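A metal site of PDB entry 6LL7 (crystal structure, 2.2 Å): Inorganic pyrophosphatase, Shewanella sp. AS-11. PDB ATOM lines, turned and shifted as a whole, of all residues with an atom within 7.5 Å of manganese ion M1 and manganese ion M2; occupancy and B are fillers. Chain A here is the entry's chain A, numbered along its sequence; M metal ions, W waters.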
ATOM      1  N   HIS A   9      32.033  10.931 -29.166  1.00  0.00           N
ATOM      2  CA  HIS A   9      32.178  12.405 -29.373  1.00  0.00           C
ATOM      3  C   HIS A   9      32.724  13.078 -28.100  1.00  0.00           C
ATOM      4  O   HIS A   9      32.604  12.515 -26.999  1.00  0.00           O
ATOM      5  CB  HIS A   9      30.850  13.053 -29.842  1.00  0.00           C
ATOM      6  CG  HIS A   9      29.641  12.751 -29.022  1.00  0.00           C
ATOM      7  ND1 HIS A   9      29.530  13.067 -27.675  1.00  0.00           N
ATOM      8  CD2 HIS A   9      28.448  12.208 -29.375  1.00  0.00           C
ATOM      9  CE1 HIS A   9      28.347  12.678 -27.220  1.00  0.00           C
ATOM     10  NE2 HIS A   9      27.655  12.168 -28.255  1.00  0.00           N
ATOM     11  N   LYS A  10      33.335  14.241 -28.317  1.00  0.00           N
ATOM     12  CA  LYS A  10      33.640  15.252 -27.275  1.00  0.00           C
ATOM     13  C   LYS A  10      32.405  15.409 -26.395  1.00  0.00           C
ATOM     14  O   LYS A  10      31.292  15.388 -26.972  1.00  0.00           O
ATOM     15  CB  LYS A  10      33.991  16.602 -27.906  1.00  0.00           C
ATOM     16  CG  LYS A  10      35.172  16.565 -28.857  1.00  0.00           C
ATOM     17  CD  LYS A  10      35.823  17.923 -29.045  1.00  0.00           C
ATOM     18  CE  LYS A  10      37.314  17.793 -29.266  1.00  0.00           C
ATOM     19  NZ  LYS A  10      37.838  18.874 -30.130  1.00  0.00           N
ATOM     20  N   ILE A  11      32.617  15.586 -25.090  1.00  0.00           N
ATOM     21  CA  ILE A  11      31.546  15.648 -24.057  1.00  0.00           C
ATOM     22  C   ILE A  11      30.760  14.349 -24.140  1.00  0.00           C
ATOM     23  O   ILE A  11      29.575  14.330 -24.439  1.00  0.00           O
ATOM     24  CB  ILE A  11      30.732  16.951 -24.195  1.00  0.00           C
ATOM     25  CG1 ILE A  11      31.693  18.153 -24.199  1.00  0.00           C
ATOM     26  CG2 ILE A  11      29.682  17.050 -23.097  1.00  0.00           C
ATOM     27  CD1 ILE A  11      31.058  19.511 -24.050  1.00  0.00           C
ATOM     28  N   PRO A  12      31.413  13.192 -23.907  1.00  0.00           N
ATOM     29  CA  PRO A  12      30.759  11.893 -24.083  1.00  0.00           C
ATOM     30  C   PRO A  12      29.452  11.716 -23.311  1.00  0.00           C
ATOM     31  O   PRO A  12      29.389  12.034 -22.144  1.00  0.00           O
ATOM     32  CB  PRO A  12      31.822  10.899 -23.556  1.00  0.00           C
ATOM     33  CG  PRO A  12      32.795  11.730 -22.762  1.00  0.00           C
ATOM     34  CD  PRO A  12      32.808  13.079 -23.456  1.00  0.00           C
ATOM     35  N   ASP A  13      28.432  11.166 -23.945  1.00  0.00           N
ATOM     36  CA  ASP A  13      27.165  10.750 -23.285  1.00  0.00           C
ATOM     37  C   ASP A  13      27.216   9.247 -23.072  1.00  0.00           C
ATOM     38  O   ASP A  13      28.243   8.649 -23.423  1.00  0.00           O
ATOM     39  CB  ASP A  13      25.941  11.159 -24.123  1.00  0.00           C
ATOM     40  CG  ASP A  13      26.028  10.704 -25.570  1.00  0.00           C
ATOM     41  OD1 ASP A  13      26.977   9.976 -25.912  1.00  0.00           O
ATOM     42  OD2 ASP A  13      25.165  11.131 -26.335  1.00  0.00           O
ATOM     43  N   SER A  14      26.148   8.629 -22.529  1.00  0.00           N
ATOM     44  CA  SER A  14      26.122   7.158 -22.289  1.00  0.00           C
ATOM     45  C   SER A  14      26.353   6.380 -23.593  1.00  0.00           C
ATOM     46  O   SER A  14      27.161   5.401 -23.554  1.00  0.00           O
ATOM     47  CB  SER A  14      24.861   6.752 -21.607  1.00  0.00           C
ATOM     48  OG  SER A  14      24.881   7.180 -20.249  1.00  0.00           O
ATOM     49  N   ASP A  15      25.737   6.809 -24.710  1.00  0.00           N
ATOM     50  CA  ASP A  15      25.849   6.139 -26.022  1.00  0.00           C
ATOM     51  C   ASP A  15      27.322   6.040 -26.430  1.00  0.00           C
ATOM     52  O   ASP A  15      27.750   4.924 -26.797  1.00  0.00           O
ATOM     53  CB  ASP A  15      25.035   6.850 -27.116  1.00  0.00           C
ATOM     54  CG  ASP A  15      24.834   6.034 -28.385  1.00  0.00           C
ATOM     55  OD1 ASP A  15      25.035   4.812 -28.326  1.00  0.00           O
ATOM     56  OD2 ASP A  15      24.428   6.635 -29.420  1.00  0.00           O
ATOM     57  N   SER A  16      28.048   7.177 -26.407  1.00  0.00           N
ATOM     58  CA  SER A  16      29.481   7.256 -26.802  1.00  0.00           C
ATOM     59  C   SER A  16      30.337   6.346 -25.906  1.00  0.00           C
ATOM     60  O   SER A  16      31.274   5.720 -26.458  1.00  0.00           O
ATOM     61  CB  SER A  16      30.021   8.663 -26.753  1.00  0.00           C
ATOM     62  OG  SER A  16      29.262   9.549 -27.588  1.00  0.00           O
ATOM     63  N   VAL A  72      32.331   6.421 -32.890  1.00  0.00           N
ATOM     64  CA  VAL A  72      30.956   6.080 -32.392  1.00  0.00           C
ATOM     65  C   VAL A  72      30.118   7.367 -32.256  1.00  0.00           C
ATOM     66  O   VAL A  72      30.633   8.355 -31.682  1.00  0.00           O
ATOM     67  CB  VAL A  72      31.022   5.339 -31.062  1.00  0.00           C
ATOM     68  CG1 VAL A  72      29.640   5.020 -30.530  1.00  0.00           C
ATOM     69  CG2 VAL A  72      31.877   4.090 -31.169  1.00  0.00           C
ATOM     70  N   ASP A  73      28.876   7.346 -32.781  1.00  0.00           N
ATOM     71  CA  ASP A  73      27.767   8.260 -32.366  1.00  0.00           C
ATOM     72  C   ASP A  73      27.983   9.671 -32.920  1.00  0.00           C
ATOM     73  O   ASP A  73      27.464  10.630 -32.317  1.00  0.00           O
ATOM     74  CB  ASP A  73      27.665   8.323 -30.835  1.00  0.00           C
ATOM     75  CG  ASP A  73      26.365   8.882 -30.269  1.00  0.00           C
ATOM     76  OD1 ASP A  73      25.339   8.828 -30.971  1.00  0.00           O
ATOM     77  OD2 ASP A  73      26.421   9.364 -29.114  1.00  0.00           O
ATOM     78  N   HIS A  74      28.754   9.804 -33.974  1.00  0.00           N
ATOM     79  CA  HIS A  74      28.808  11.035 -34.818  1.00  0.00           C
ATOM     80  C   HIS A  74      29.498  10.704 -36.155  1.00  0.00           C
ATOM     81  O   HIS A  74      30.038   9.603 -36.276  1.00  0.00           O
ATOM     82  CB  HIS A  74      29.522  12.167 -34.077  1.00  0.00           C
ATOM     83  CG  HIS A  74      30.979  11.912 -33.873  1.00  0.00           C
ATOM     84  ND1 HIS A  74      31.930  12.414 -34.759  1.00  0.00           N
ATOM     85  CD2 HIS A  74      31.658  11.261 -32.908  1.00  0.00           C
ATOM     86  CE1 HIS A  74      33.118  12.049 -34.338  1.00  0.00           C
ATOM     87  NE2 HIS A  74      32.990  11.356 -33.207  1.00  0.00           N
ATOM     88  N   GLN A  79      33.155  17.152 -33.570  1.00  0.00           N
ATOM     89  CA  GLN A  79      32.919  16.202 -32.459  1.00  0.00           C
ATOM     90  C   GLN A  79      34.021  15.150 -32.381  1.00  0.00           C
ATOM     91  O   GLN A  79      34.051  14.402 -31.396  1.00  0.00           O
ATOM     92  CB  GLN A  79      31.541  15.566 -32.609  1.00  0.00           C
ATOM     93  CG  GLN A  79      30.423  16.461 -32.074  1.00  0.00           C
ATOM     94  CD  GLN A  79      29.114  15.715 -32.008  1.00  0.00           C
ATOM     95  OE1 GLN A  79      28.694  15.236 -30.954  1.00  0.00           O
ATOM     96  NE2 GLN A  79      28.466  15.613 -33.161  1.00  0.00           N
ATOM     97  N   ASP A  94      27.054   4.838 -36.160  1.00  0.00           N
ATOM     98  CA  ASP A  94      26.289   6.055 -35.794  1.00  0.00           C
ATOM     99  C   ASP A  94      24.830   5.925 -36.247  1.00  0.00           C
ATOM    100  O   ASP A  94      24.490   4.960 -36.959  1.00  0.00           O
ATOM    101  CB  ASP A  94      26.953   7.288 -36.419  1.00  0.00           C
ATOM    102  CG  ASP A  94      26.367   8.610 -35.965  1.00  0.00           C
ATOM    103  OD1 ASP A  94      25.695   8.624 -34.897  1.00  0.00           O
ATOM    104  OD2 ASP A  94      26.591   9.625 -36.674  1.00  0.00           O
ATOM    105  N   HIS A  95      24.013   6.906 -35.853  1.00  0.00           N
ATOM    106  CA  HIS A  95      22.579   7.015 -36.209  1.00  0.00           C
ATOM    107  C   HIS A  95      22.249   8.478 -36.486  1.00  0.00           C
ATOM    108  O   HIS A  95      21.077   8.854 -36.301  1.00  0.00           O
ATOM    109  CB  HIS A  95      21.715   6.451 -35.078  1.00  0.00           C
ATOM    110  CG  HIS A  95      21.879   7.141 -33.767  1.00  0.00           C
ATOM    111  ND1 HIS A  95      20.909   7.964 -33.229  1.00  0.00           N
ATOM    112  CD2 HIS A  95      22.910   7.155 -32.893  1.00  0.00           C
ATOM    113  CE1 HIS A  95      21.331   8.443 -32.072  1.00  0.00           C
ATOM    114  NE2 HIS A  95      22.564   7.949 -31.843  1.00  0.00           N
ATOM    115  N   HIS A  96      23.225   9.282 -36.921  1.00  0.00           N
ATOM    116  CA  HIS A  96      23.008  10.697 -37.320  1.00  0.00           C
ATOM    117  C   HIS A  96      23.132  10.843 -38.832  1.00  0.00           C
ATOM    118  O   HIS A  96      23.568   9.885 -39.521  1.00  0.00           O
ATOM    119  CB  HIS A  96      24.007  11.624 -36.639  1.00  0.00           C
ATOM    120  CG  HIS A  96      23.832  11.647 -35.157  1.00  0.00           C
ATOM    121  ND1 HIS A  96      24.547  10.818 -34.306  1.00  0.00           N
ATOM    122  CD2 HIS A  96      23.018  12.398 -34.367  1.00  0.00           C
ATOM    123  CE1 HIS A  96      24.168  11.042 -33.063  1.00  0.00           C
ATOM    124  NE2 HIS A  96      23.245  12.027 -33.085  1.00  0.00           N
ATOM    125  N   VAL A 114      18.132   5.233 -36.730  1.00  0.00           N
ATOM    126  CA  VAL A 114      17.585   4.734 -35.446  1.00  0.00           C
ATOM    127  C   VAL A 114      17.933   5.770 -34.372  1.00  0.00           C
ATOM    128  O   VAL A 114      18.522   6.823 -34.738  1.00  0.00           O
ATOM    129  CB  VAL A 114      18.111   3.334 -35.101  1.00  0.00           C
ATOM    130  CG1 VAL A 114      17.624   2.319 -36.112  1.00  0.00           C
ATOM    131  CG2 VAL A 114      19.631   3.292 -34.986  1.00  0.00           C
ATOM    132  N   GLY A 115      17.541   5.510 -33.135  1.00  0.00           N
ATOM    133  CA  GLY A 115      17.663   6.458 -32.018  1.00  0.00           C
ATOM    134  C   GLY A 115      18.940   6.294 -31.208  1.00  0.00           C
ATOM    135  O   GLY A 115      19.131   7.099 -30.266  1.00  0.00           O
ATOM    136  N   CYS A 116      19.794   5.317 -31.541  1.00  0.00           N
ATOM    137  CA  CYS A 116      20.970   4.966 -30.709  1.00  0.00           C
ATOM    138  C   CYS A 116      22.013   4.110 -31.438  1.00  0.00           C
ATOM    139  O   CYS A 116      21.651   3.029 -31.965  1.00  0.00           O
ATOM    140  CB  CYS A 116      20.506   4.222 -29.469  1.00  0.00           C
ATOM    141  SG  CYS A 116      21.746   4.166 -28.153  1.00  0.00           S
ATOM    142  N   SER A 117      23.287   4.519 -31.358  1.00  0.00           N
ATOM    143  CA  SER A 117      24.452   3.788 -31.913  1.00  0.00           C
ATOM    144  C   SER A 117      24.473   2.353 -31.384  1.00  0.00           C
ATOM    145  O   SER A 117      24.802   1.421 -32.127  1.00  0.00           O
ATOM    146  CB  SER A 117      25.743   4.509 -31.631  1.00  0.00           C
ATOM    147  OG  SER A 117      25.660   5.894 -31.909  1.00  0.00           O
ATOM    148  N   ASN A 118      24.083   2.174 -30.126  1.00  0.00           N
ATOM    149  CA  ASN A 118      24.141   0.865 -29.433  1.00  0.00           C
ATOM    150  C   ASN A 118      23.113  -0.089 -30.081  1.00  0.00           C
ATOM    151  O   ASN A 118      23.305  -1.279 -30.023  1.00  0.00           O
ATOM    152  CB  ASN A 118      24.017   1.062 -27.921  1.00  0.00           C
ATOM    153  CG  ASN A 118      25.359   1.231 -27.267  1.00  0.00           C
ATOM    154  OD1 ASN A 118      25.950   0.257 -26.796  1.00  0.00           O
ATOM    155  ND2 ASN A 118      25.894   2.446 -27.237  1.00  0.00           N
ATOM    156  N   ALA A 143      22.206   2.640 -22.608  1.00  0.00           N
ATOM    157  CA  ALA A 143      22.569   3.623 -23.649  1.00  0.00           C
ATOM    158  C   ALA A 143      21.331   3.923 -24.501  1.00  0.00           C
ATOM    159  O   ALA A 143      21.107   5.117 -24.804  1.00  0.00           O
ATOM    160  CB  ALA A 143      23.694   3.129 -24.505  1.00  0.00           C
ATOM    161  N   ASP A 147      19.384   7.524 -24.731  1.00  0.00           N
ATOM    162  CA  ASP A 147      19.241   8.206 -26.032  1.00  0.00           C
ATOM    163  C   ASP A 147      17.765   8.423 -26.381  1.00  0.00           C
ATOM    164  O   ASP A 147      17.441   9.529 -26.870  1.00  0.00           O
ATOM    165  CB  ASP A 147      19.920   7.413 -27.169  1.00  0.00           C
ATOM    166  CG  ASP A 147      21.222   8.017 -27.695  1.00  0.00           C
ATOM    167  OD1 ASP A 147      21.493   9.161 -27.306  1.00  0.00           O
ATOM    168  OD2 ASP A 147      21.942   7.340 -28.517  1.00  0.00           O
ATOM    169  N   ASP A 202      25.930  18.383 -21.028  1.00  0.00           N
ATOM    170  CA  ASP A 202      25.685  18.038 -22.454  1.00  0.00           C
ATOM    171  C   ASP A 202      25.479  19.338 -23.248  1.00  0.00           C
ATOM    172  O   ASP A 202      24.318  19.660 -23.580  1.00  0.00           O
ATOM    173  CB  ASP A 202      24.472  17.115 -22.603  1.00  0.00           C
ATOM    174  CG  ASP A 202      24.236  16.677 -24.033  1.00  0.00           C
ATOM    175  OD1 ASP A 202      25.231  16.476 -24.752  1.00  0.00           O
ATOM    176  OD2 ASP A 202      23.057  16.577 -24.437  1.00  0.00           O
ATOM    177  N   LYS A 204      26.684  21.812 -26.651  1.00  0.00           N
ATOM    178  CA  LYS A 204      27.177  21.813 -28.051  1.00  0.00           C
ATOM    179  C   LYS A 204      27.129  23.222 -28.624  1.00  0.00           C
ATOM    180  O   LYS A 204      26.178  23.961 -28.318  1.00  0.00           O
ATOM    181  CB  LYS A 204      26.321  20.894 -28.909  1.00  0.00           C
ATOM    182  CG  LYS A 204      26.637  19.412 -28.790  1.00  0.00           C
ATOM    183  CD  LYS A 204      25.780  18.614 -29.751  1.00  0.00           C
ATOM    184  CE  LYS A 204      26.093  17.133 -29.746  1.00  0.00           C
ATOM    185  NZ  LYS A 204      25.538  16.461 -30.934  1.00  0.00           N
ATOM    186  N   ARG A 294      16.965  17.617 -28.647  1.00  0.00           N
ATOM    187  CA  ARG A 294      17.690  18.801 -29.172  1.00  0.00           C
ATOM    188  C   ARG A 294      17.821  18.693 -30.692  1.00  0.00           C
ATOM    189  O   ARG A 294      17.536  19.682 -31.381  1.00  0.00           O
ATOM    190  CB  ARG A 294      19.075  18.954 -28.528  1.00  0.00           C
ATOM    191  CG  ARG A 294      19.834  20.173 -29.050  1.00  0.00           C
ATOM    192  CD  ARG A 294      21.078  20.509 -28.246  1.00  0.00           C
ATOM    193  NE  ARG A 294      21.917  19.335 -28.101  1.00  0.00           N
ATOM    194  CZ  ARG A 294      22.761  19.104 -27.092  1.00  0.00           C
ATOM    195  NH1 ARG A 294      22.943  19.971 -26.110  1.00  0.00           N
ATOM    196  NH2 ARG A 294      23.465  17.989 -27.076  1.00  0.00           N
ATOM    197  N   LYS A 295      18.253  17.535 -31.221  1.00  0.00           N
ATOM    198  CA  LYS A 295      18.626  17.422 -32.667  1.00  0.00           C
ATOM    199  C   LYS A 295      17.369  17.381 -33.542  1.00  0.00           C
ATOM    200  O   LYS A 295      17.506  17.648 -34.741  1.00  0.00           O
ATOM    201  CB  LYS A 295      19.582  16.249 -32.936  1.00  0.00           C
ATOM    202  CG  LYS A 295      18.973  14.853 -32.927  1.00  0.00           C
ATOM    203  CD  LYS A 295      19.582  13.888 -33.912  1.00  0.00           C
ATOM    204  CE  LYS A 295      19.100  12.465 -33.712  1.00  0.00           C
ATOM    205  NZ  LYS A 295      19.444  11.976 -32.344  1.00  0.00           N
HETATM  206 MN    MN M   1      23.510   8.557 -29.895  1.00  0.00          MN
HETATM  207 MN    MN M   2      25.609  11.227 -28.290  1.00  0.00          MN
HETATM  208  O   HOH W   1      22.854  10.830 -29.354  1.00  0.00           O
HETATM  209  O   HOH W   2      25.074  11.540 -30.064  1.00  0.00           O
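Manganese ion M2 is bound by water W2 (1.9 Å), the side-chain carboxylate of Asp 13 (2.0 Å), the side-chain carboxylate of Asp 73 (2.2 Å) and a ring nitrogen (NE2) of His 9 (2.3 Å).
OD1 of Asp 13 is in hydrogen-bond range of OG of Ser 16, 2.9 Å away.
OG of Ser 16 sits close to OD2 of Asp 73 (3.2 Å).
The side-chain carboxylate of Asp 15 lies close to the side-chain hydroxyl of Ser 117 (2.9 Å).
The side-chain amide nitrogen (ND2) of Asn 118 lies within hydrogen-bond range of the side-chain carboxylate (OD1) of Asp 15 (2.7 Å).
ND1 of His 95 is in hydrogen-bond range of N of Cys 116 (3.3 Å).
O of Val 114 lies within hydrogen-bond range of ND1 of His 95 (3.0 Å).
The backbone NH of His 9 sits close to the side-chain hydroxyl of Ser 16, at 3.5 Å.
A ring nitrogen (ND1) of His 9 sits close to the backbone carbonyl oxygen (O) of Ile 11, 3.5 Å away.
Ser 117 touches manganese ion M1 (OG to MN, 3.97 Å).
Of the 26 residues printed, 5 come within 4 Å of manganese ion M1.
Along chain A the residues within 4 Å of manganese ion M1 span positions 15 to 147.
The nearest printed residue that does not touch manganese ion M1 is His 96 (4.1 Å).
Manganese ion M1 is bound by OD1 of Asp 73 (2.1 Å), OD2 of Asp 15 (2.2 Å), NE2 of His 95 (2.2 Å), OD2 of Asp 147 (2.4 Å) and water W1 (2.4 Å).
Manganese ion M1 has five donor atoms within binding distance.
Within 4 Å of manganese ion M2: His 9, Asp 13 and Asp 73.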
